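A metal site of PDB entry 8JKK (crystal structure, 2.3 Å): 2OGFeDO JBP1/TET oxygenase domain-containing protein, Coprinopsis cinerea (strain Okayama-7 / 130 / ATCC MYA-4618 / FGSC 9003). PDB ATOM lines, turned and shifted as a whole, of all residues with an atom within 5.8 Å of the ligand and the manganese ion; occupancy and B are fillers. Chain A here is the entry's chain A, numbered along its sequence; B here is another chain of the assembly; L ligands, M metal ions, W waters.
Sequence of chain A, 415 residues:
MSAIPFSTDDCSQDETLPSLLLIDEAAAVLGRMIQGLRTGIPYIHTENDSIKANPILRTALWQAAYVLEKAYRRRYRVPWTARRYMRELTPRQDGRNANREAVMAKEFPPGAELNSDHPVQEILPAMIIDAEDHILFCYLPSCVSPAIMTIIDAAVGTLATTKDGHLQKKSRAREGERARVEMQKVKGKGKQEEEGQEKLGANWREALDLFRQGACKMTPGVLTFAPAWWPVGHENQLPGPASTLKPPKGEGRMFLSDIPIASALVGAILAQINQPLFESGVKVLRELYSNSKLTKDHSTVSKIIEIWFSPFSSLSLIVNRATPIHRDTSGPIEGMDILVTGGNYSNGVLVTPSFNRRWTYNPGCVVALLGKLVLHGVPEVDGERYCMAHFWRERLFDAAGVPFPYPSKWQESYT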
ATOM      1  N   TRP A 204      24.367  28.290  -9.415  1.00  0.00           N
ATOM      2  CA  TRP A 204      24.084  26.867  -9.491  1.00  0.00           C
ATOM      3  C   TRP A 204      22.601  26.555  -9.371  1.00  0.00           C
ATOM      4  O   TRP A 204      22.139  25.525  -9.884  1.00  0.00           O
ATOM      5  CB  TRP A 204      24.902  26.126  -8.427  1.00  0.00           C
ATOM      6  CG  TRP A 204      24.406  26.337  -7.035  1.00  0.00           C
ATOM      7  CD1 TRP A 204      24.895  27.230  -6.120  1.00  0.00           C
ATOM      8  CD2 TRP A 204      23.338  25.634  -6.385  1.00  0.00           C
ATOM      9  NE1 TRP A 204      24.194  27.130  -4.939  1.00  0.00           N
ATOM     10  CE2 TRP A 204      23.248  26.153  -5.067  1.00  0.00           C
ATOM     11  CE3 TRP A 204      22.461  24.616  -6.773  1.00  0.00           C
ATOM     12  CZ2 TRP A 204      22.301  25.699  -4.140  1.00  0.00           C
ATOM     13  CZ3 TRP A 204      21.513  24.163  -5.846  1.00  0.00           C
ATOM     14  CH2 TRP A 204      21.447  24.703  -4.548  1.00  0.00           C
ATOM     15  N   ARG A 205      21.831  27.415  -8.706  1.00  0.00           N
ATOM     16  CA  ARG A 205      20.421  27.105  -8.494  1.00  0.00           C
ATOM     17  C   ARG A 205      19.628  27.021  -9.791  1.00  0.00           C
ATOM     18  O   ARG A 205      18.580  26.375  -9.823  1.00  0.00           O
ATOM     19  CB  ARG A 205      19.776  28.131  -7.565  1.00  0.00           C
ATOM     20  CG  ARG A 205      20.257  28.018  -6.140  1.00  0.00           C
ATOM     21  CD  ARG A 205      19.643  29.099  -5.282  1.00  0.00           C
ATOM     22  NE  ARG A 205      20.318  29.205  -3.993  1.00  0.00           N
ATOM     23  CZ  ARG A 205      20.123  28.365  -2.977  1.00  0.00           C
ATOM     24  NH1 ARG A 205      19.272  27.348  -3.109  1.00  0.00           N
ATOM     25  NH2 ARG A 205      20.767  28.544  -1.842  1.00  0.00           N
ATOM     26  N   ILE A 318      11.153  24.761  -6.763  1.00  0.00           N
ATOM     27  CA  ILE A 318      12.201  24.241  -7.625  1.00  0.00           C
ATOM     28  C   ILE A 318      11.589  23.066  -8.388  1.00  0.00           C
ATOM     29  O   ILE A 318      11.277  22.027  -7.785  1.00  0.00           O
ATOM     30  CB  ILE A 318      13.435  23.794  -6.815  1.00  0.00           C
ATOM     31  CG1 ILE A 318      14.030  24.954  -6.012  1.00  0.00           C
ATOM     32  CG2 ILE A 318      14.512  23.192  -7.706  1.00  0.00           C
ATOM     33  CD1 ILE A 318      13.512  25.047  -4.612  1.00  0.00           C
ATOM     34  N   ARG A 321      14.511  19.786 -10.871  1.00  0.00           N
ATOM     35  CA  ARG A 321      15.924  20.107 -10.769  1.00  0.00           C
ATOM     36  C   ARG A 321      16.594  19.243  -9.713  1.00  0.00           C
ATOM     37  O   ARG A 321      16.127  19.168  -8.574  1.00  0.00           O
ATOM     38  CB  ARG A 321      16.134  21.601 -10.445  1.00  0.00           C
ATOM     39  CG  ARG A 321      17.578  22.091 -10.690  1.00  0.00           C
ATOM     40  CD  ARG A 321      17.956  23.263  -9.755  1.00  0.00           C
ATOM     41  NE  ARG A 321      18.048  22.847  -8.355  1.00  0.00           N
ATOM     42  CZ  ARG A 321      17.877  23.655  -7.320  1.00  0.00           C
ATOM     43  NH1 ARG A 321      17.625  24.952  -7.507  1.00  0.00           N
ATOM     44  NH2 ARG A 321      17.943  23.169  -6.099  1.00  0.00           N
ATOM     45  N   ALA A 322      17.712  18.624 -10.100  1.00  0.00           N
ATOM     46  CA  ALA A 322      18.562  17.995  -9.113  1.00  0.00           C
ATOM     47  C   ALA A 322      19.263  19.070  -8.277  1.00  0.00           C
ATOM     48  O   ALA A 322      19.382  20.229  -8.685  1.00  0.00           O
ATOM     49  CB  ALA A 322      19.586  17.082  -9.788  1.00  0.00           C
ATOM     50  N   THR A 323      19.721  18.678  -7.093  1.00  0.00           N
ATOM     51  CA  THR A 323      20.286  19.613  -6.131  1.00  0.00           C
ATOM     52  C   THR A 323      21.637  19.110  -5.635  1.00  0.00           C
ATOM     53  O   THR A 323      21.683  18.151  -4.838  1.00  0.00           O
ATOM     54  CB  THR A 323      19.311  19.795  -4.964  1.00  0.00           C
ATOM     55  OG1 THR A 323      18.073  20.305  -5.465  1.00  0.00           O
ATOM     56  CG2 THR A 323      19.865  20.776  -3.906  1.00  0.00           C
ATOM     57  N   HIS A 326      25.116  21.140  -0.769  1.00  0.00           N
ATOM     58  CA  HIS A 326      25.339  22.561  -0.508  1.00  0.00           C
ATOM     59  C   HIS A 326      24.837  22.898   0.892  1.00  0.00           C
ATOM     60  O   HIS A 326      24.125  22.133   1.526  1.00  0.00           O
ATOM     61  CB  HIS A 326      24.600  23.438  -1.523  1.00  0.00           C
ATOM     62  CG  HIS A 326      23.121  23.454  -1.291  1.00  0.00           C
ATOM     63  ND1 HIS A 326      22.316  22.385  -1.614  1.00  0.00           N
ATOM     64  CD2 HIS A 326      22.318  24.357  -0.676  1.00  0.00           C
ATOM     65  CE1 HIS A 326      21.077  22.646  -1.251  1.00  0.00           C
ATOM     66  NE2 HIS A 326      21.051  23.836  -0.668  1.00  0.00           N
ATOM     67  N   ARG A 327      25.234  24.082   1.361  1.00  0.00           N
ATOM     68  CA  ARG A 327      24.546  24.791   2.427  1.00  0.00           C
ATOM     69  C   ARG A 327      23.938  26.055   1.839  1.00  0.00           C
ATOM     70  O   ARG A 327      24.459  26.617   0.884  1.00  0.00           O
ATOM     71  CB  ARG A 327      25.489  25.193   3.562  1.00  0.00           C
ATOM     72  CG  ARG A 327      26.218  24.065   4.255  1.00  0.00           C
ATOM     73  CD  ARG A 327      27.104  24.620   5.388  1.00  0.00           C
ATOM     74  NE  ARG A 327      28.009  23.624   5.971  1.00  0.00           N
ATOM     75  CZ  ARG A 327      29.209  23.328   5.474  1.00  0.00           C
ATOM     76  NH1 ARG A 327      29.634  23.951   4.389  1.00  0.00           N
ATOM     77  NH2 ARG A 327      29.997  22.427   6.063  1.00  0.00           N
ATOM     78  N   ASP A 328      22.812  26.489   2.404  1.00  0.00           N
ATOM     79  CA  ASP A 328      22.153  27.728   2.044  1.00  0.00           C
ATOM     80  C   ASP A 328      22.662  28.822   2.963  1.00  0.00           C
ATOM     81  O   ASP A 328      22.488  28.734   4.184  1.00  0.00           O
ATOM     82  CB  ASP A 328      20.623  27.590   2.172  1.00  0.00           C
ATOM     83  CG  ASP A 328      20.066  26.448   1.343  1.00  0.00           C
ATOM     84  OD1 ASP A 328      20.089  26.559   0.088  1.00  0.00           O
ATOM     85  OD2 ASP A 328      19.592  25.449   1.920  1.00  0.00           O
ATOM     86  N   LEU A 339      11.774  21.670   3.783  1.00  0.00           N
ATOM     87  CA  LEU A 339      11.678  21.175   2.417  1.00  0.00           C
ATOM     88  C   LEU A 339      10.498  20.232   2.335  1.00  0.00           C
ATOM     89  O   LEU A 339      10.295  19.401   3.227  1.00  0.00           O
ATOM     90  CB  LEU A 339      12.958  20.420   2.046  1.00  0.00           C
ATOM     91  CG  LEU A 339      14.248  21.219   2.278  1.00  0.00           C
ATOM     92  CD1 LEU A 339      15.470  20.338   2.123  1.00  0.00           C
ATOM     93  CD2 LEU A 339      14.287  22.378   1.261  1.00  0.00           C
ATOM     94  N   VAL A 340       9.700  20.397   1.267  1.00  0.00           N
ATOM     95  CA  VAL A 340       8.630  19.460   0.916  1.00  0.00           C
ATOM     96  C   VAL A 340       8.905  18.997  -0.503  1.00  0.00           C
ATOM     97  O   VAL A 340       9.164  19.830  -1.378  1.00  0.00           O
ATOM     98  CB  VAL A 340       7.250  20.108   1.010  1.00  0.00           C
ATOM     99  CG1 VAL A 340       6.146  19.051   0.827  1.00  0.00           C
ATOM    100  CG2 VAL A 340       7.090  20.799   2.342  1.00  0.00           C
ATOM    101  N   THR A 341       8.877  17.696  -0.739  1.00  0.00           N
ATOM    102  CA  THR A 341       9.142  17.182  -2.083  1.00  0.00           C
ATOM    103  C   THR A 341       7.927  16.433  -2.614  1.00  0.00           C
ATOM    104  O   THR A 341       7.216  15.762  -1.847  1.00  0.00           O
ATOM    105  CB  THR A 341      10.401  16.277  -2.099  1.00  0.00           C
ATOM    106  OG1 THR A 341      10.681  15.876  -3.452  1.00  0.00           O
ATOM    107  CG2 THR A 341      10.222  15.017  -1.193  1.00  0.00           C
ATOM    108  N   LEU A 350      17.790  12.067  -0.172  1.00  0.00           N
ATOM    109  CA  LEU A 350      18.412  13.281   0.315  1.00  0.00           C
ATOM    110  C   LEU A 350      19.663  12.909   1.089  1.00  0.00           C
ATOM    111  O   LEU A 350      19.602  12.072   2.012  1.00  0.00           O
ATOM    112  CB  LEU A 350      17.440  14.103   1.169  1.00  0.00           C
ATOM    113  CG  LEU A 350      17.896  15.529   1.552  1.00  0.00           C
ATOM    114  CD1 LEU A 350      16.708  16.462   1.626  1.00  0.00           C
ATOM    115  CD2 LEU A 350      18.495  15.462   2.908  1.00  0.00           C
ATOM    116  N   TYR A 361      13.485   9.971   0.238  1.00  0.00           N
ATOM    117  CA  TYR A 361      12.988  11.315   0.002  1.00  0.00           C
ATOM    118  C   TYR A 361      11.991  11.277  -1.154  1.00  0.00           C
ATOM    119  O   TYR A 361      12.181  11.897  -2.201  1.00  0.00           O
ATOM    120  CB  TYR A 361      14.161  12.239  -0.269  1.00  0.00           C
ATOM    121  CG  TYR A 361      13.894  13.733  -0.285  1.00  0.00           C
ATOM    122  CD1 TYR A 361      13.467  14.409   0.850  1.00  0.00           C
ATOM    123  CD2 TYR A 361      14.123  14.477  -1.429  1.00  0.00           C
ATOM    124  CE1 TYR A 361      13.248  15.788   0.821  1.00  0.00           C
ATOM    125  CE2 TYR A 361      13.930  15.850  -1.454  1.00  0.00           C
ATOM    126  CZ  TYR A 361      13.497  16.496  -0.327  1.00  0.00           C
ATOM    127  OH  TYR A 361      13.305  17.852  -0.381  1.00  0.00           O
ATOM    128  N   GLY A 371      19.594  24.609   7.362  1.00  0.00           N
ATOM    129  CA  GLY A 371      20.202  24.512   6.045  1.00  0.00           C
ATOM    130  C   GLY A 371      21.476  25.335   5.858  1.00  0.00           C
ATOM    131  O   GLY A 371      22.138  25.169   4.829  1.00  0.00           O
ATOM    132  N   HIS A 376      23.397  19.391   2.446  1.00  0.00           N
ATOM    133  CA  HIS A 376      22.328  18.512   1.957  1.00  0.00           C
ATOM    134  C   HIS A 376      22.292  18.540   0.429  1.00  0.00           C
ATOM    135  O   HIS A 376      22.635  19.549  -0.187  1.00  0.00           O
ATOM    136  CB  HIS A 376      20.949  18.901   2.513  1.00  0.00           C
ATOM    137  CG  HIS A 376      20.603  20.355   2.328  1.00  0.00           C
ATOM    138  ND1 HIS A 376      21.192  21.358   3.063  1.00  0.00           N
ATOM    139  CD2 HIS A 376      19.731  20.962   1.492  1.00  0.00           C
ATOM    140  CE1 HIS A 376      20.693  22.526   2.702  1.00  0.00           C
ATOM    141  NE2 HIS A 376      19.806  22.319   1.749  1.00  0.00           N
ATOM    142  N   VAL A 378      20.161  16.461  -3.214  1.00  0.00           N
ATOM    143  CA  VAL A 378      19.159  15.554  -3.751  1.00  0.00           C
ATOM    144  C   VAL A 378      19.546  15.179  -5.184  1.00  0.00           C
ATOM    145  O   VAL A 378      19.433  16.010  -6.089  1.00  0.00           O
ATOM    146  CB  VAL A 378      17.747  16.163  -3.708  1.00  0.00           C
ATOM    147  CG1 VAL A 378      16.721  15.150  -4.168  1.00  0.00           C
ATOM    148  CG2 VAL A 378      17.425  16.672  -2.331  1.00  0.00           C
ATOM    149  N   ARG A 385       9.654  15.711 -10.460  1.00  0.00           N
ATOM    150  CA  ARG A 385       9.750  16.084  -9.053  1.00  0.00           C
ATOM    151  C   ARG A 385       9.682  17.601  -8.942  1.00  0.00           C
ATOM    152  O   ARG A 385      10.091  18.326  -9.857  1.00  0.00           O
ATOM    153  CB  ARG A 385      11.058  15.563  -8.450  1.00  0.00           C
ATOM    154  CG  ARG A 385      11.329  15.994  -7.034  1.00  0.00           C
ATOM    155  CD  ARG A 385      12.540  15.305  -6.458  1.00  0.00           C
ATOM    156  NE  ARG A 385      13.735  16.104  -6.644  1.00  0.00           N
ATOM    157  CZ  ARG A 385      14.084  17.108  -5.840  1.00  0.00           C
ATOM    158  NH1 ARG A 385      13.308  17.422  -4.790  1.00  0.00           N
ATOM    159  NH2 ARG A 385      15.181  17.805  -6.080  1.00  0.00           N
ATOM    160  N   TYR A 386       9.151  18.061  -7.812  1.00  0.00           N
ATOM    161  CA  TYR A 386       9.271  19.464  -7.441  1.00  0.00           C
ATOM    162  C   TYR A 386       9.571  19.527  -5.947  1.00  0.00           C
ATOM    163  O   TYR A 386       9.305  18.587  -5.194  1.00  0.00           O
ATOM    164  CB  TYR A 386       8.012  20.276  -7.751  1.00  0.00           C
ATOM    165  CG  TYR A 386       6.780  19.759  -7.040  1.00  0.00           C
ATOM    166  CD1 TYR A 386       6.560  20.042  -5.688  1.00  0.00           C
ATOM    167  CD2 TYR A 386       5.844  18.973  -7.712  1.00  0.00           C
ATOM    168  CE1 TYR A 386       5.451  19.563  -5.034  1.00  0.00           C
ATOM    169  CE2 TYR A 386       4.720  18.483  -7.069  1.00  0.00           C
ATOM    170  CZ  TYR A 386       4.536  18.785  -5.734  1.00  0.00           C
ATOM    171  OH  TYR A 386       3.451  18.307  -5.087  1.00  0.00           O
ATOM    172  N   CYS A 387      10.114  20.669  -5.534  1.00  0.00           N
ATOM    173  CA  CYS A 387      10.446  20.922  -4.134  1.00  0.00           C
ATOM    174  C   CYS A 387       9.946  22.303  -3.745  1.00  0.00           C
ATOM    175  O   CYS A 387      10.147  23.275  -4.499  1.00  0.00           O
ATOM    176  CB  CYS A 387      11.963  20.821  -3.907  1.00  0.00           C
ATOM    177  SG  CYS A 387      12.512  21.569  -2.352  1.00  0.00           S
ATOM    178  N   ALA A 389      10.720  24.914  -0.886  1.00  0.00           N
ATOM    179  CA  ALA A 389      11.717  25.221   0.134  1.00  0.00           C
ATOM    180  C   ALA A 389      11.310  26.503   0.849  1.00  0.00           C
ATOM    181  O   ALA A 389      11.188  27.566   0.224  1.00  0.00           O
ATOM    182  CB  ALA A 389      13.101  25.359  -0.511  1.00  0.00           C
ATOM    183  N1  5CM B   6      17.237  31.242  -2.449  1.00  0.00           N
ATOM    184  C2  5CM B   6      17.701  31.569  -1.200  1.00  0.00           C
ATOM    185  N3  5CM B   6      17.632  30.770  -0.170  1.00  0.00           N
ATOM    186  C4  5CM B   6      17.117  29.612  -0.232  1.00  0.00           C
ATOM    187  C5  5CM B   6      16.601  29.180  -1.499  1.00  0.00           C
ATOM    188  C5A 5CM B   6      16.001  27.800  -1.603  1.00  0.00           C
ATOM    189  C6  5CM B   6      16.686  30.038  -2.582  1.00  0.00           C
ATOM    190  O2  5CM B   6      18.206  32.623  -0.967  1.00  0.00           O
ATOM    191  N4  5CM B   6      17.100  28.876   0.849  1.00  0.00           N
ATOM    192  C1' 5CM B   6      17.312  32.143  -3.588  1.00  0.00           C
ATOM    193  C2' 5CM B   6      16.909  33.620  -3.378  1.00  0.00           C
ATOM    194  C3' 5CM B   6      17.934  34.477  -4.069  1.00  0.00           C
ATOM    195  C4' 5CM B   6      18.993  33.439  -4.373  1.00  0.00           C
ATOM    196  O4' 5CM B   6      18.635  32.163  -3.896  1.00  0.00           O
ATOM    197  O3' 5CM B   6      17.187  34.545  -5.191  1.00  0.00           O
ATOM    198  C5' 5CM B   6      20.369  33.851  -3.899  1.00  0.00           C
ATOM    199  O5' 5CM B   6      20.831  33.386  -2.677  1.00  0.00           O
ATOM    200  P   5CM B   6      22.368  32.975  -2.549  1.00  0.00           P
ATOM    201  OP1 5CM B   6      22.548  32.970  -1.105  1.00  0.00           O
ATOM    202  OP2 5CM B   6      22.694  31.824  -3.379  1.00  0.00           O
HETATM  203  C1  LIG L   1      17.560  23.983  -2.305  1.00  0.00           C
HETATM  204  C2  LIG L   1      17.304  22.599  -1.712  1.00  0.00           C
HETATM  205  C3  LIG L   1      16.076  20.431  -1.928  1.00  0.00           C
HETATM  206  C4  LIG L   1      15.374  19.689  -3.069  1.00  0.00           C
HETATM  207  O1  LIG L   1      18.137  24.855  -1.609  1.00  0.00           O
HETATM  208  O2  LIG L   1      17.214  24.229  -3.491  1.00  0.00           O
HETATM  209  O3  LIG L   1      17.899  22.289  -0.659  1.00  0.00           O
HETATM  210  O4  LIG L   1      14.518  18.833  -2.740  1.00  0.00           O
HETATM  211  N1  LIG L   1      16.436  21.797  -2.373  1.00  0.00           N
HETATM  212  O5  LIG L   1      15.682  19.994  -4.242  1.00  0.00           O
HETATM  213 MN    MN M   1      19.034  24.063   0.170  1.00  0.00          MN
HETATM  214  O   HOH W   1      17.226  24.291   1.310  1.00  0.00           O
HETATM  215  O   HOH W   2      17.421  26.359  -5.154  1.00  0.00           O
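Ile 318 touches the ligand (CD1 to O2, 3.95 Å). CG2 of Val 378 touches O4 of the ligand (3.6 Å). 5CM 6 of chain B touches the ligand (C5A to O1, 3.6 Å). Hydrophobic or aromatic side chains within 4 Å of the ligand: Ile 318, His 326, Tyr 361, His 376 and Val 378. 12 residues have an atom within 4 Å of the ligand: Arg 205, Ile 318, Arg 321, Thr 323, His 326, Asp 328, Tyr 361, His 376, Val 378, Arg 385, Cys 387 and 5CM 6 of chain B. The nearest printed residue that does not touch the ligand is Leu 339 (4.1 Å).
An oxygen (O4) of the ligand sits at hydrogen-bond distance from the side-chain hydroxyl (OH) of Tyr 361, at 2.8 Å. The guanidinium group (NH2) of Arg 321 lies within salt-bridge range of an oxygen (O2) of the ligand (2.9 Å). The side-chain hydroxyl (OG1) of Thr 323 is in hydrogen-bond range of an oxygen (O5) of the ligand. O4 of the ligand lies within hydrogen-bond range of SG of Cys 387. O4 of the ligand is in salt-bridge range of NH1 of Arg 385, 2.8 Å away. The guanidinium group of Arg 205 is in salt-bridge range of an oxygen (O2) of the ligand (3.8 Å).
Water W2 lies within hydrogen-bond range of an oxygen (O2) of the ligand (2.7 Å), the guanidinium group of Arg 321 (2.7 Å) and the guanidinium group of Arg 205 (2.9 Å).
The manganese ion is bound by an oxygen (O1) of the ligand (2.1 Å), water W1 (2.1 Å), a ring nitrogen (NE2) of His 326 (2.2 Å), an oxygen (O3) of the ligand (2.3 Å), the side-chain carboxylate of Asp 328 (2.3 Å) and a ring nitrogen (NE2) of His 376 (2.5 Å). The manganese ion has six donor atoms within binding distance. Slightly farther from the manganese ion lies the side-chain carboxylate (OD1) of Asp 328 (2.7 Å).
O of Arg 205 sits at hydrogen-bond distance from NH1 of Arg 321 (2.9 Å). The backbone NH of Cys 387 lies within hydrogen-bond range of the backbone carbonyl oxygen of Ile 318 (2.9 Å). N of Asp 328 is in hydrogen-bond range of O of Gly 371, at 2.8 Å. The side-chain carboxylate of Asp 328 lies within salt-bridge range of the guanidinium group of Arg 205, at 2.9 Å. The backbone carbonyl oxygen (O) of Thr 323 sits at hydrogen-bond distance from the backbone NH (N) of Val 378 (2.8 Å). The side-chain hydroxyl of Thr 341 is in hydrogen-bond range of the guanidinium group of Arg 385 (3.3 Å). OP2 of 5CM 6 of chain B lies within salt-bridge range of the guanidinium group (NE) of Arg 205 (3.6 Å). The side-chain hydroxyl (OG1) of Thr 323 sits at hydrogen-bond distance from the guanidinium group (NH2) of Arg 321.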
